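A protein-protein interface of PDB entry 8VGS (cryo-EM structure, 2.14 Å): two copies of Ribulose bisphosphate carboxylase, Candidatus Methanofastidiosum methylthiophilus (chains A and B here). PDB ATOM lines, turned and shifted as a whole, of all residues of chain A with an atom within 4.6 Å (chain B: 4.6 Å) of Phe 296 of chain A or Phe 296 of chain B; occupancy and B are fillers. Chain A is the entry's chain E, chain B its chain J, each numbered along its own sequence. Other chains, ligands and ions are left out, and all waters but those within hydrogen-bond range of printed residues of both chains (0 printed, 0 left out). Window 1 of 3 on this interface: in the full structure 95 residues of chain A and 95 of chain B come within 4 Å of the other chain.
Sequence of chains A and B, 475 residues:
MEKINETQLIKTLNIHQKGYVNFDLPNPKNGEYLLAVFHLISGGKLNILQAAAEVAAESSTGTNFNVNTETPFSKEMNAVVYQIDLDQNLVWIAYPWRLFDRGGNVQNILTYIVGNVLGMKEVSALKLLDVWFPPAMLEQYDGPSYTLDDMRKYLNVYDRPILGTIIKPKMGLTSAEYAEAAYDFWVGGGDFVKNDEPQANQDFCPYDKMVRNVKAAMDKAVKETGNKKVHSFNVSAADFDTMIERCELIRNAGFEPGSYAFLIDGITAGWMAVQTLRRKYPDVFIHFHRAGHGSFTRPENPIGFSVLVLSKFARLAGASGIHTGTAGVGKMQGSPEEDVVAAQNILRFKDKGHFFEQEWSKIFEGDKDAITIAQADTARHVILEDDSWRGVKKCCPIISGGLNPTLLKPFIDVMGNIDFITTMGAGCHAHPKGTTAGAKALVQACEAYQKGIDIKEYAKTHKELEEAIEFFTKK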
ATOM      1  N   LEU A 118      -8.098 -25.386 -21.226  1.00  0.00           N
ATOM      2  CA  LEU A 118      -7.754 -25.354 -19.809  1.00  0.00           C
ATOM      3  C   LEU A 118      -8.812 -24.627 -18.989  1.00  0.00           C
ATOM      4  O   LEU A 118      -8.999 -24.935 -17.807  1.00  0.00           O
ATOM      5  CB  LEU A 118      -6.388 -24.694 -19.618  1.00  0.00           C
ATOM      6  CG  LEU A 118      -5.235 -25.297 -20.424  1.00  0.00           C
ATOM      7  CD1 LEU A 118      -3.933 -24.566 -20.134  1.00  0.00           C
ATOM      8  CD2 LEU A 118      -5.097 -26.783 -20.136  1.00  0.00           C
ATOM      9  N   LYS A 127      -4.653 -32.373 -18.443  1.00  0.00           N
ATOM     10  CA  LYS A 127      -3.200 -32.219 -18.473  1.00  0.00           C
ATOM     11  C   LYS A 127      -2.658 -32.859 -19.743  1.00  0.00           C
ATOM     12  O   LYS A 127      -2.779 -34.072 -19.929  1.00  0.00           O
ATOM     13  CB  LYS A 127      -2.556 -32.842 -17.235  1.00  0.00           C
ATOM     14  CG  LYS A 127      -1.152 -32.340 -16.949  1.00  0.00           C
ATOM     15  CD  LYS A 127      -1.178 -31.150 -16.005  1.00  0.00           C
ATOM     16  CE  LYS A 127       0.107 -31.049 -15.201  1.00  0.00           C
ATOM     17  NZ  LYS A 127       0.175 -29.779 -14.426  1.00  0.00           N
ATOM     18  N   ILE A 267       8.170 -18.390 -20.491  1.00  0.00           N
ATOM     19  CA  ILE A 267       6.780 -18.420 -20.049  1.00  0.00           C
ATOM     20  C   ILE A 267       6.227 -17.004 -19.927  1.00  0.00           C
ATOM     21  O   ILE A 267       5.179 -16.679 -20.496  1.00  0.00           O
ATOM     22  CB  ILE A 267       6.655 -19.191 -18.723  1.00  0.00           C
ATOM     23  CG1 ILE A 267       7.135 -20.634 -18.898  1.00  0.00           C
ATOM     24  CG2 ILE A 267       5.219 -19.165 -18.228  1.00  0.00           C
ATOM     25  CD1 ILE A 267       6.701 -21.273 -20.199  1.00  0.00           C
ATOM     26  N   GLY A 292       7.750 -19.536 -14.047  1.00  0.00           N
ATOM     27  CA  GLY A 292       6.309 -19.525 -14.159  1.00  0.00           C
ATOM     28  C   GLY A 292       5.706 -20.767 -14.778  1.00  0.00           C
ATOM     29  O   GLY A 292       4.475 -20.855 -14.872  1.00  0.00           O
ATOM     30  N   HIS A 293       6.530 -21.731 -15.199  1.00  0.00           N
ATOM     31  CA  HIS A 293       6.026 -22.942 -15.839  1.00  0.00           C
ATOM     32  C   HIS A 293       5.245 -23.835 -14.886  1.00  0.00           C
ATOM     33  O   HIS A 293       4.493 -24.697 -15.355  1.00  0.00           O
ATOM     34  CB  HIS A 293       7.184 -23.751 -16.425  1.00  0.00           C
ATOM     35  CG  HIS A 293       7.922 -24.568 -15.408  1.00  0.00           C
ATOM     36  ND1 HIS A 293       7.726 -25.925 -15.263  1.00  0.00           N
ATOM     37  CD2 HIS A 293       8.833 -24.218 -14.469  1.00  0.00           C
ATOM     38  CE1 HIS A 293       8.497 -26.377 -14.289  1.00  0.00           C
ATOM     39  NE2 HIS A 293       9.177 -25.361 -13.790  1.00  0.00           N
ATOM     40  N   GLY A 294       5.412 -23.645 -13.571  1.00  0.00           N
ATOM     41  CA  GLY A 294       4.926 -24.620 -12.602  1.00  0.00           C
ATOM     42  C   GLY A 294       3.426 -24.829 -12.647  1.00  0.00           C
ATOM     43  O   GLY A 294       2.949 -25.964 -12.562  1.00  0.00           O
ATOM     44  N   SER A 295       2.664 -23.742 -12.816  1.00  0.00           N
ATOM     45  CA  SER A 295       1.212 -23.844 -12.928  1.00  0.00           C
ATOM     46  C   SER A 295       0.796 -24.720 -14.102  1.00  0.00           C
ATOM     47  O   SER A 295      -0.229 -25.409 -14.030  1.00  0.00           O
ATOM     48  CB  SER A 295       0.595 -22.455 -13.069  1.00  0.00           C
ATOM     49  OG  SER A 295       0.977 -21.616 -11.995  1.00  0.00           O
ATOM     50  N   PHE A 296       1.576 -24.716 -15.183  1.00  0.00           N
ATOM     51  CA  PHE A 296       1.307 -25.636 -16.280  1.00  0.00           C
ATOM     52  C   PHE A 296       1.724 -27.060 -15.928  1.00  0.00           C
ATOM     53  O   PHE A 296       1.018 -28.017 -16.261  1.00  0.00           O
ATOM     54  CB  PHE A 296       2.023 -25.173 -17.549  1.00  0.00           C
ATOM     55  CG  PHE A 296       1.517 -23.869 -18.094  1.00  0.00           C
ATOM     56  CD1 PHE A 296       0.199 -23.732 -18.501  1.00  0.00           C
ATOM     57  CD2 PHE A 296       2.365 -22.782 -18.218  1.00  0.00           C
ATOM     58  CE1 PHE A 296      -0.264 -22.536 -19.009  1.00  0.00           C
ATOM     59  CE2 PHE A 296       1.908 -21.583 -18.726  1.00  0.00           C
ATOM     60  CZ  PHE A 296       0.591 -21.459 -19.123  1.00  0.00           C
ATOM     61  N   THR A 297       2.855 -27.222 -15.236  1.00  0.00           N
ATOM     62  CA  THR A 297       3.534 -28.512 -15.191  1.00  0.00           C
ATOM     63  C   THR A 297       3.550 -29.180 -13.825  1.00  0.00           C
ATOM     64  O   THR A 297       3.934 -30.353 -13.744  1.00  0.00           O
ATOM     65  CB  THR A 297       4.983 -28.367 -15.678  1.00  0.00           C
ATOM     66  OG1 THR A 297       5.721 -27.568 -14.746  1.00  0.00           O
ATOM     67  CG2 THR A 297       5.030 -27.717 -17.051  1.00  0.00           C
ATOM     68  N   ARG A 298       3.180 -28.478 -12.760  1.00  0.00           N
ATOM     69  CA  ARG A 298       3.225 -29.068 -11.427  1.00  0.00           C
ATOM     70  C   ARG A 298       2.239 -30.229 -11.330  1.00  0.00           C
ATOM     71  O   ARG A 298       1.089 -30.097 -11.771  1.00  0.00           O
ATOM     72  CB  ARG A 298       2.908 -28.020 -10.361  1.00  0.00           C
ATOM     73  CG  ARG A 298       4.071 -27.097 -10.017  1.00  0.00           C
ATOM     74  CD  ARG A 298       5.158 -27.829  -9.251  1.00  0.00           C
ATOM     75  NE  ARG A 298       4.713 -28.248  -7.928  1.00  0.00           N
ATOM     76  CZ  ARG A 298       4.926 -27.564  -6.812  1.00  0.00           C
ATOM     77  NH1 ARG A 298       5.565 -26.405  -6.823  1.00  0.00           N
ATOM     78  NH2 ARG A 298       4.489 -28.055  -5.656  1.00  0.00           N
ATOM     79  N   ILE A 303      -4.645 -29.279 -14.182  1.00  0.00           N
ATOM     80  CA  ILE A 303      -4.877 -28.629 -15.466  1.00  0.00           C
ATOM     81  C   ILE A 303      -3.582 -27.970 -15.918  1.00  0.00           C
ATOM     82  O   ILE A 303      -3.018 -27.135 -15.202  1.00  0.00           O
ATOM     83  CB  ILE A 303      -6.020 -27.604 -15.379  1.00  0.00           C
ATOM     84  CG1 ILE A 303      -7.355 -28.323 -15.174  1.00  0.00           C
ATOM     85  CG2 ILE A 303      -6.059 -26.741 -16.634  1.00  0.00           C
ATOM     86  CD1 ILE A 303      -8.405 -27.479 -14.500  1.00  0.00           C
ATOM     87  N   GLY A 304      -3.117 -28.345 -17.100  1.00  0.00           N
ATOM     88  CA  GLY A 304      -1.886 -27.804 -17.654  1.00  0.00           C
ATOM     89  C   GLY A 304      -1.306 -28.761 -18.680  1.00  0.00           C
ATOM     90  O   GLY A 304      -2.039 -29.466 -19.373  1.00  0.00           O
ATOM     91  N   PHE A 305       0.022 -28.763 -18.759  1.00  0.00           N
ATOM     92  CA  PHE A 305       0.742 -29.699 -19.608  1.00  0.00           C
ATOM     93  C   PHE A 305       2.054 -30.074 -18.935  1.00  0.00           C
ATOM     94  O   PHE A 305       2.601 -29.324 -18.124  1.00  0.00           O
ATOM     95  CB  PHE A 305       0.976 -29.130 -21.020  1.00  0.00           C
ATOM     96  CG  PHE A 305       1.630 -27.773 -21.045  1.00  0.00           C
ATOM     97  CD1 PHE A 305       3.010 -27.644 -20.988  1.00  0.00           C
ATOM     98  CD2 PHE A 305       0.863 -26.627 -21.155  1.00  0.00           C
ATOM     99  CE1 PHE A 305       3.605 -26.397 -21.019  1.00  0.00           C
ATOM    100  CE2 PHE A 305       1.455 -25.380 -21.191  1.00  0.00           C
ATOM    101  CZ  PHE A 305       2.826 -25.264 -21.121  1.00  0.00           C
ATOM    102  N   LEU B 118       6.444 -20.944  -8.272  1.00  0.00           N
ATOM    103  CA  LEU B 118       5.441 -21.956  -8.586  1.00  0.00           C
ATOM    104  C   LEU B 118       6.053 -23.348  -8.682  1.00  0.00           C
ATOM    105  O   LEU B 118       5.389 -24.339  -8.365  1.00  0.00           O
ATOM    106  CB  LEU B 118       4.728 -21.600  -9.890  1.00  0.00           C
ATOM    107  CG  LEU B 118       4.138 -20.191  -9.975  1.00  0.00           C
ATOM    108  CD1 LEU B 118       3.514 -19.942 -11.339  1.00  0.00           C
ATOM    109  CD2 LEU B 118       3.121 -19.970  -8.868  1.00  0.00           C
ATOM    110  N   LYS B 127      -0.897 -19.874  -4.607  1.00  0.00           N
ATOM    111  CA  LYS B 127      -1.769 -19.143  -5.522  1.00  0.00           C
ATOM    112  C   LYS B 127      -1.736 -17.662  -5.175  1.00  0.00           C
ATOM    113  O   LYS B 127      -2.114 -17.275  -4.065  1.00  0.00           O
ATOM    114  CB  LYS B 127      -3.198 -19.682  -5.466  1.00  0.00           C
ATOM    115  CG  LYS B 127      -4.031 -19.342  -6.689  1.00  0.00           C
ATOM    116  CD  LYS B 127      -4.020 -20.480  -7.693  1.00  0.00           C
ATOM    117  CE  LYS B 127      -5.246 -20.444  -8.587  1.00  0.00           C
ATOM    118  NZ  LYS B 127      -5.145 -21.434  -9.694  1.00  0.00           N
ATOM    119  N   ILE B 267      -1.308 -14.947 -23.018  1.00  0.00           N
ATOM    120  CA  ILE B 267      -0.620 -16.002 -22.284  1.00  0.00           C
ATOM    121  C   ILE B 267       0.394 -16.709 -23.179  1.00  0.00           C
ATOM    122  O   ILE B 267       1.549 -16.918 -22.792  1.00  0.00           O
ATOM    123  CB  ILE B 267      -1.635 -16.991 -21.685  1.00  0.00           C
ATOM    124  CG1 ILE B 267      -2.584 -16.264 -20.732  1.00  0.00           C
ATOM    125  CG2 ILE B 267      -0.919 -18.122 -20.961  1.00  0.00           C
ATOM    126  CD1 ILE B 267      -1.910 -15.200 -19.892  1.00  0.00           C
ATOM    127  N   GLY B 292      -5.135 -20.221 -22.553  1.00  0.00           N
ATOM    128  CA  GLY B 292      -4.097 -20.856 -21.771  1.00  0.00           C
ATOM    129  C   GLY B 292      -3.984 -20.374 -20.341  1.00  0.00           C
ATOM    130  O   GLY B 292      -3.148 -20.898 -19.593  1.00  0.00           O
ATOM    131  N   HIS B 293      -4.798 -19.394 -19.935  1.00  0.00           N
ATOM    132  CA  HIS B 293      -4.720 -18.845 -18.586  1.00  0.00           C
ATOM    133  C   HIS B 293      -5.151 -19.838 -17.515  1.00  0.00           C
ATOM    134  O   HIS B 293      -4.808 -19.638 -16.343  1.00  0.00           O
ATOM    135  CB  HIS B 293      -5.593 -17.593 -18.475  1.00  0.00           C
ATOM    136  CG  HIS B 293      -7.053 -17.888 -18.315  1.00  0.00           C
ATOM    137  ND1 HIS B 293      -7.701 -17.802 -17.102  1.00  0.00           N
ATOM    138  CD2 HIS B 293      -7.987 -18.292 -19.210  1.00  0.00           C
ATOM    139  CE1 HIS B 293      -8.972 -18.124 -17.259  1.00  0.00           C
ATOM    140  NE2 HIS B 293      -9.171 -18.428 -18.528  1.00  0.00           N
ATOM    141  N   GLY B 294      -5.881 -20.894 -17.897  1.00  0.00           N
ATOM    142  CA  GLY B 294      -6.575 -21.723 -16.919  1.00  0.00           C
ATOM    143  C   GLY B 294      -5.652 -22.391 -15.918  1.00  0.00           C
ATOM    144  O   GLY B 294      -5.957 -22.443 -14.724  1.00  0.00           O
ATOM    145  N   SER B 295      -4.498 -22.880 -16.388  1.00  0.00           N
ATOM    146  CA  SER B 295      -3.523 -23.503 -15.496  1.00  0.00           C
ATOM    147  C   SER B 295      -3.053 -22.542 -14.413  1.00  0.00           C
ATOM    148  O   SER B 295      -2.758 -22.967 -13.290  1.00  0.00           O
ATOM    149  CB  SER B 295      -2.326 -24.016 -16.295  1.00  0.00           C
ATOM    150  OG  SER B 295      -2.741 -24.859 -17.353  1.00  0.00           O
ATOM    151  N   PHE B 296      -2.984 -21.247 -14.724  1.00  0.00           N
ATOM    152  CA  PHE B 296      -2.707 -20.260 -13.688  1.00  0.00           C
ATOM    153  C   PHE B 296      -3.917 -20.044 -12.786  1.00  0.00           C
ATOM    154  O   PHE B 296      -3.776 -19.969 -11.561  1.00  0.00           O
ATOM    155  CB  PHE B 296      -2.279 -18.936 -14.322  1.00  0.00           C
ATOM    156  CG  PHE B 296      -0.965 -19.001 -15.047  1.00  0.00           C
ATOM    157  CD1 PHE B 296       0.188 -19.385 -14.386  1.00  0.00           C
ATOM    158  CD2 PHE B 296      -0.883 -18.666 -16.387  1.00  0.00           C
ATOM    159  CE1 PHE B 296       1.399 -19.441 -15.049  1.00  0.00           C
ATOM    160  CE2 PHE B 296       0.324 -18.719 -17.055  1.00  0.00           C
ATOM    161  CZ  PHE B 296       1.467 -19.107 -16.385  1.00  0.00           C
ATOM    162  N   THR B 297      -5.115 -19.960 -13.369  1.00  0.00           N
ATOM    163  CA  THR B 297      -6.248 -19.352 -12.683  1.00  0.00           C
ATOM    164  C   THR B 297      -7.343 -20.322 -12.263  1.00  0.00           C
ATOM    165  O   THR B 297      -8.249 -19.910 -11.530  1.00  0.00           O
ATOM    166  CB  THR B 297      -6.877 -18.262 -13.564  1.00  0.00           C
ATOM    167  OG1 THR B 297      -7.439 -18.863 -14.735  1.00  0.00           O
ATOM    168  CG2 THR B 297      -5.835 -17.237 -13.976  1.00  0.00           C
ATOM    169  N   ARG B 298      -7.308 -21.571 -12.712  1.00  0.00           N
ATOM    170  CA  ARG B 298      -8.366 -22.507 -12.356  1.00  0.00           C
ATOM    171  C   ARG B 298      -8.341 -22.791 -10.857  1.00  0.00           C
ATOM    172  O   ARG B 298      -7.260 -22.999 -10.288  1.00  0.00           O
ATOM    173  CB  ARG B 298      -8.230 -23.812 -13.140  1.00  0.00           C
ATOM    174  CG  ARG B 298      -8.664 -23.720 -14.596  1.00  0.00           C
ATOM    175  CD  ARG B 298     -10.177 -23.663 -14.722  1.00  0.00           C
ATOM    176  NE  ARG B 298     -10.819 -24.899 -14.289  1.00  0.00           N
ATOM    177  CZ  ARG B 298     -11.242 -25.854 -15.108  1.00  0.00           C
ATOM    178  NH1 ARG B 298     -11.089 -25.760 -16.418  1.00  0.00           N
ATOM    179  NH2 ARG B 298     -11.832 -26.931 -14.597  1.00  0.00           N
ATOM    180  N   ILE B 303      -1.629 -24.113  -7.649  1.00  0.00           N
ATOM    181  CA  ILE B 303      -0.458 -23.294  -7.939  1.00  0.00           C
ATOM    182  C   ILE B 303      -0.766 -22.411  -9.138  1.00  0.00           C
ATOM    183  O   ILE B 303      -1.133 -22.909 -10.209  1.00  0.00           O
ATOM    184  CB  ILE B 303       0.788 -24.157  -8.194  1.00  0.00           C
ATOM    185  CG1 ILE B 303       1.281 -24.777  -6.885  1.00  0.00           C
ATOM    186  CG2 ILE B 303       1.887 -23.330  -8.847  1.00  0.00           C
ATOM    187  CD1 ILE B 303       1.872 -26.157  -7.044  1.00  0.00           C
ATOM    188  N   GLY B 304      -0.619 -21.107  -8.958  1.00  0.00           N
ATOM    189  CA  GLY B 304      -0.865 -20.150 -10.025  1.00  0.00           C
ATOM    190  C   GLY B 304      -1.190 -18.783  -9.446  1.00  0.00           C
ATOM    191  O   GLY B 304      -0.708 -18.420  -8.373  1.00  0.00           O
ATOM    192  N   PHE B 305      -2.009 -18.041 -10.186  1.00  0.00           N
ATOM    193  CA  PHE B 305      -2.516 -16.760  -9.721  1.00  0.00           C
ATOM    194  C   PHE B 305      -3.960 -16.600 -10.176  1.00  0.00           C
ATOM    195  O   PHE B 305      -4.399 -17.208 -11.154  1.00  0.00           O
ATOM    196  CB  PHE B 305      -1.643 -15.584 -10.201  1.00  0.00           C
ATOM    197  CG  PHE B 305      -1.377 -15.569 -11.683  1.00  0.00           C
ATOM    198  CD1 PHE B 305      -2.287 -15.008 -12.566  1.00  0.00           C
ATOM    199  CD2 PHE B 305      -0.198 -16.090 -12.190  1.00  0.00           C
ATOM    200  CE1 PHE B 305      -2.035 -14.989 -13.925  1.00  0.00           C
ATOM    201  CE2 PHE B 305       0.060 -16.069 -13.548  1.00  0.00           C
ATOM    202  CZ  PHE B 305      -0.860 -15.520 -14.416  1.00  0.00           C
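The side-chain hydroxyl (OG) of Ser 295 of chain A is in hydrogen-bond range of the backbone carbonyl oxygen (O) of Ile 303 of chain B, 3.1 Å away.
The backbone carbonyl oxygen of Ile 303 of chain A sits at hydrogen-bond distance from the side-chain hydroxyl of Ser 295 of chain B (3.1 Å).
The backbone carbonyl oxygen of Leu 118 of chain A lies within hydrogen-bond range of the guanidinium group of Arg 298 of chain B (2.6 Å).
The backbone carbonyl oxygen (O) of Leu 118 of chain B is in hydrogen-bond range of the guanidinium group (NH1) of Arg 298 of chain A (2.6 Å).
The backbone NH (N) of Gly 304 of chain B lies close to the side-chain hydroxyl (OG) of Ser 295 of chain A.
O of Arg 298 of chain A sits at hydrogen-bond distance from NZ of Lys 127 of chain A (2.8 Å).
NZ of Lys 127 of chain A is in hydrogen-bond range of O of Phe 296 of chain A (2.7 Å).
O of Phe 296 of chain B is in hydrogen-bond range of N of Phe 305 of chain B (3.0 Å).
O of Phe 296 of chain A sits at hydrogen-bond distance from N of Phe 305 of chain A.
NZ of Lys 127 of chain B lies within hydrogen-bond range of O of Phe 296 of chain B (2.7 Å).
The backbone carbonyl oxygen (O) of Arg 298 of chain B lies within hydrogen-bond range of the side-chain amino group (NZ) of Lys 127 of chain B (2.7 Å).
CD1 of Leu 118 of chain A touches O of Gly 292 of chain B, 3.8 Å away.
Gly 292 of chain A touches Leu 118 of chain B (O to CD1, 3.8 Å).
Gly 292 of chain A touches Phe 296 of chain B (O to CE1, 3.4 Å).
Leu 118 of chain B touches Ser 295 of chain A.
O of Ser 295 of chain A touches CB of Ser 295 of chain B, 3.4 Å away.
Ser 295 of chain A touches Phe 296 of chain B (OG to CD1, 3.4 Å).
CD1 of Phe 296 of chain A touches OG of Ser 295 of chain B, at 3.4 Å.
Phe 296 of chain A touches Phe 296 of chain B (CE2 to CZ, 3.4 Å).
Arg 298 of chain A touches Ile 303 of chain B (CZ to CD1, 3.4 Å).
Gly 304 of chain A touches Ser 295 of chain B (CA to OG, 3.1 Å).
Printed residues of chain B within 4 Å of Ser 295 of chain A: Leu 118, Ser 295, Phe 296, Ile 303 and Gly 304.
Of chain B, only Gly 292, Ser 295 and Phe 296 come within 4 Å of Phe 296 of chain A.
Of the printed residues of chain B, Gly 304 of chain A touches Ser 295 (3.1 Å).
Printed residues of chain A within 4 Å of Leu 118 of chain B: Gly 292, Ser 295 and Arg 298.
Gly 294 of chain B touches none of the printed residues of chain A.
Phe 296 of chain B touches three residues of chain A.
Of the printed residues of chain A, Gly 304 of chain B touches Ser 295.
Phe 305 of chain B touches none of the printed residues of chain A.
The nearest residue of chain A that does not touch Phe 296 of chain B is Ile 267 of chain A (4.2 Å).
Of the 13 printed residues of chain B, 7 touch a printed residue of chain A.
Printed residues of chain B that touch a printed residue of chain A: Leu 118, Gly 292, Ser 295, Phe 296, Arg 298, Ile 303 and Gly 304.
Leu 118 of chain A touches Gly 292 of chain B, and with the chains exchanged Gly 292 of chain A touches Leu 118 of chain B.
Leu 118 of chain A touches Ser 295 of chain B, and with the chains exchanged Ser 295 of chain A touches Leu 118 of chain B.
Leu 118 of chain A touches Arg 298 of chain B, and with the chains exchanged Arg 298 of chain A touches Leu 118 of chain B.
Gly 292 of chain A touches Phe 296 of chain B, and with the chains exchanged Phe 296 of chain A touches Gly 292 of chain B.
Positions printed for both chains: 118, 127, 267, 292, 293, 294, 295, 296, 297, 298, 303, 304 and 305.
Of the 18 pairs that touch across the chains among the printed residues, 18 have their exchanged pair printed and touching as well.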
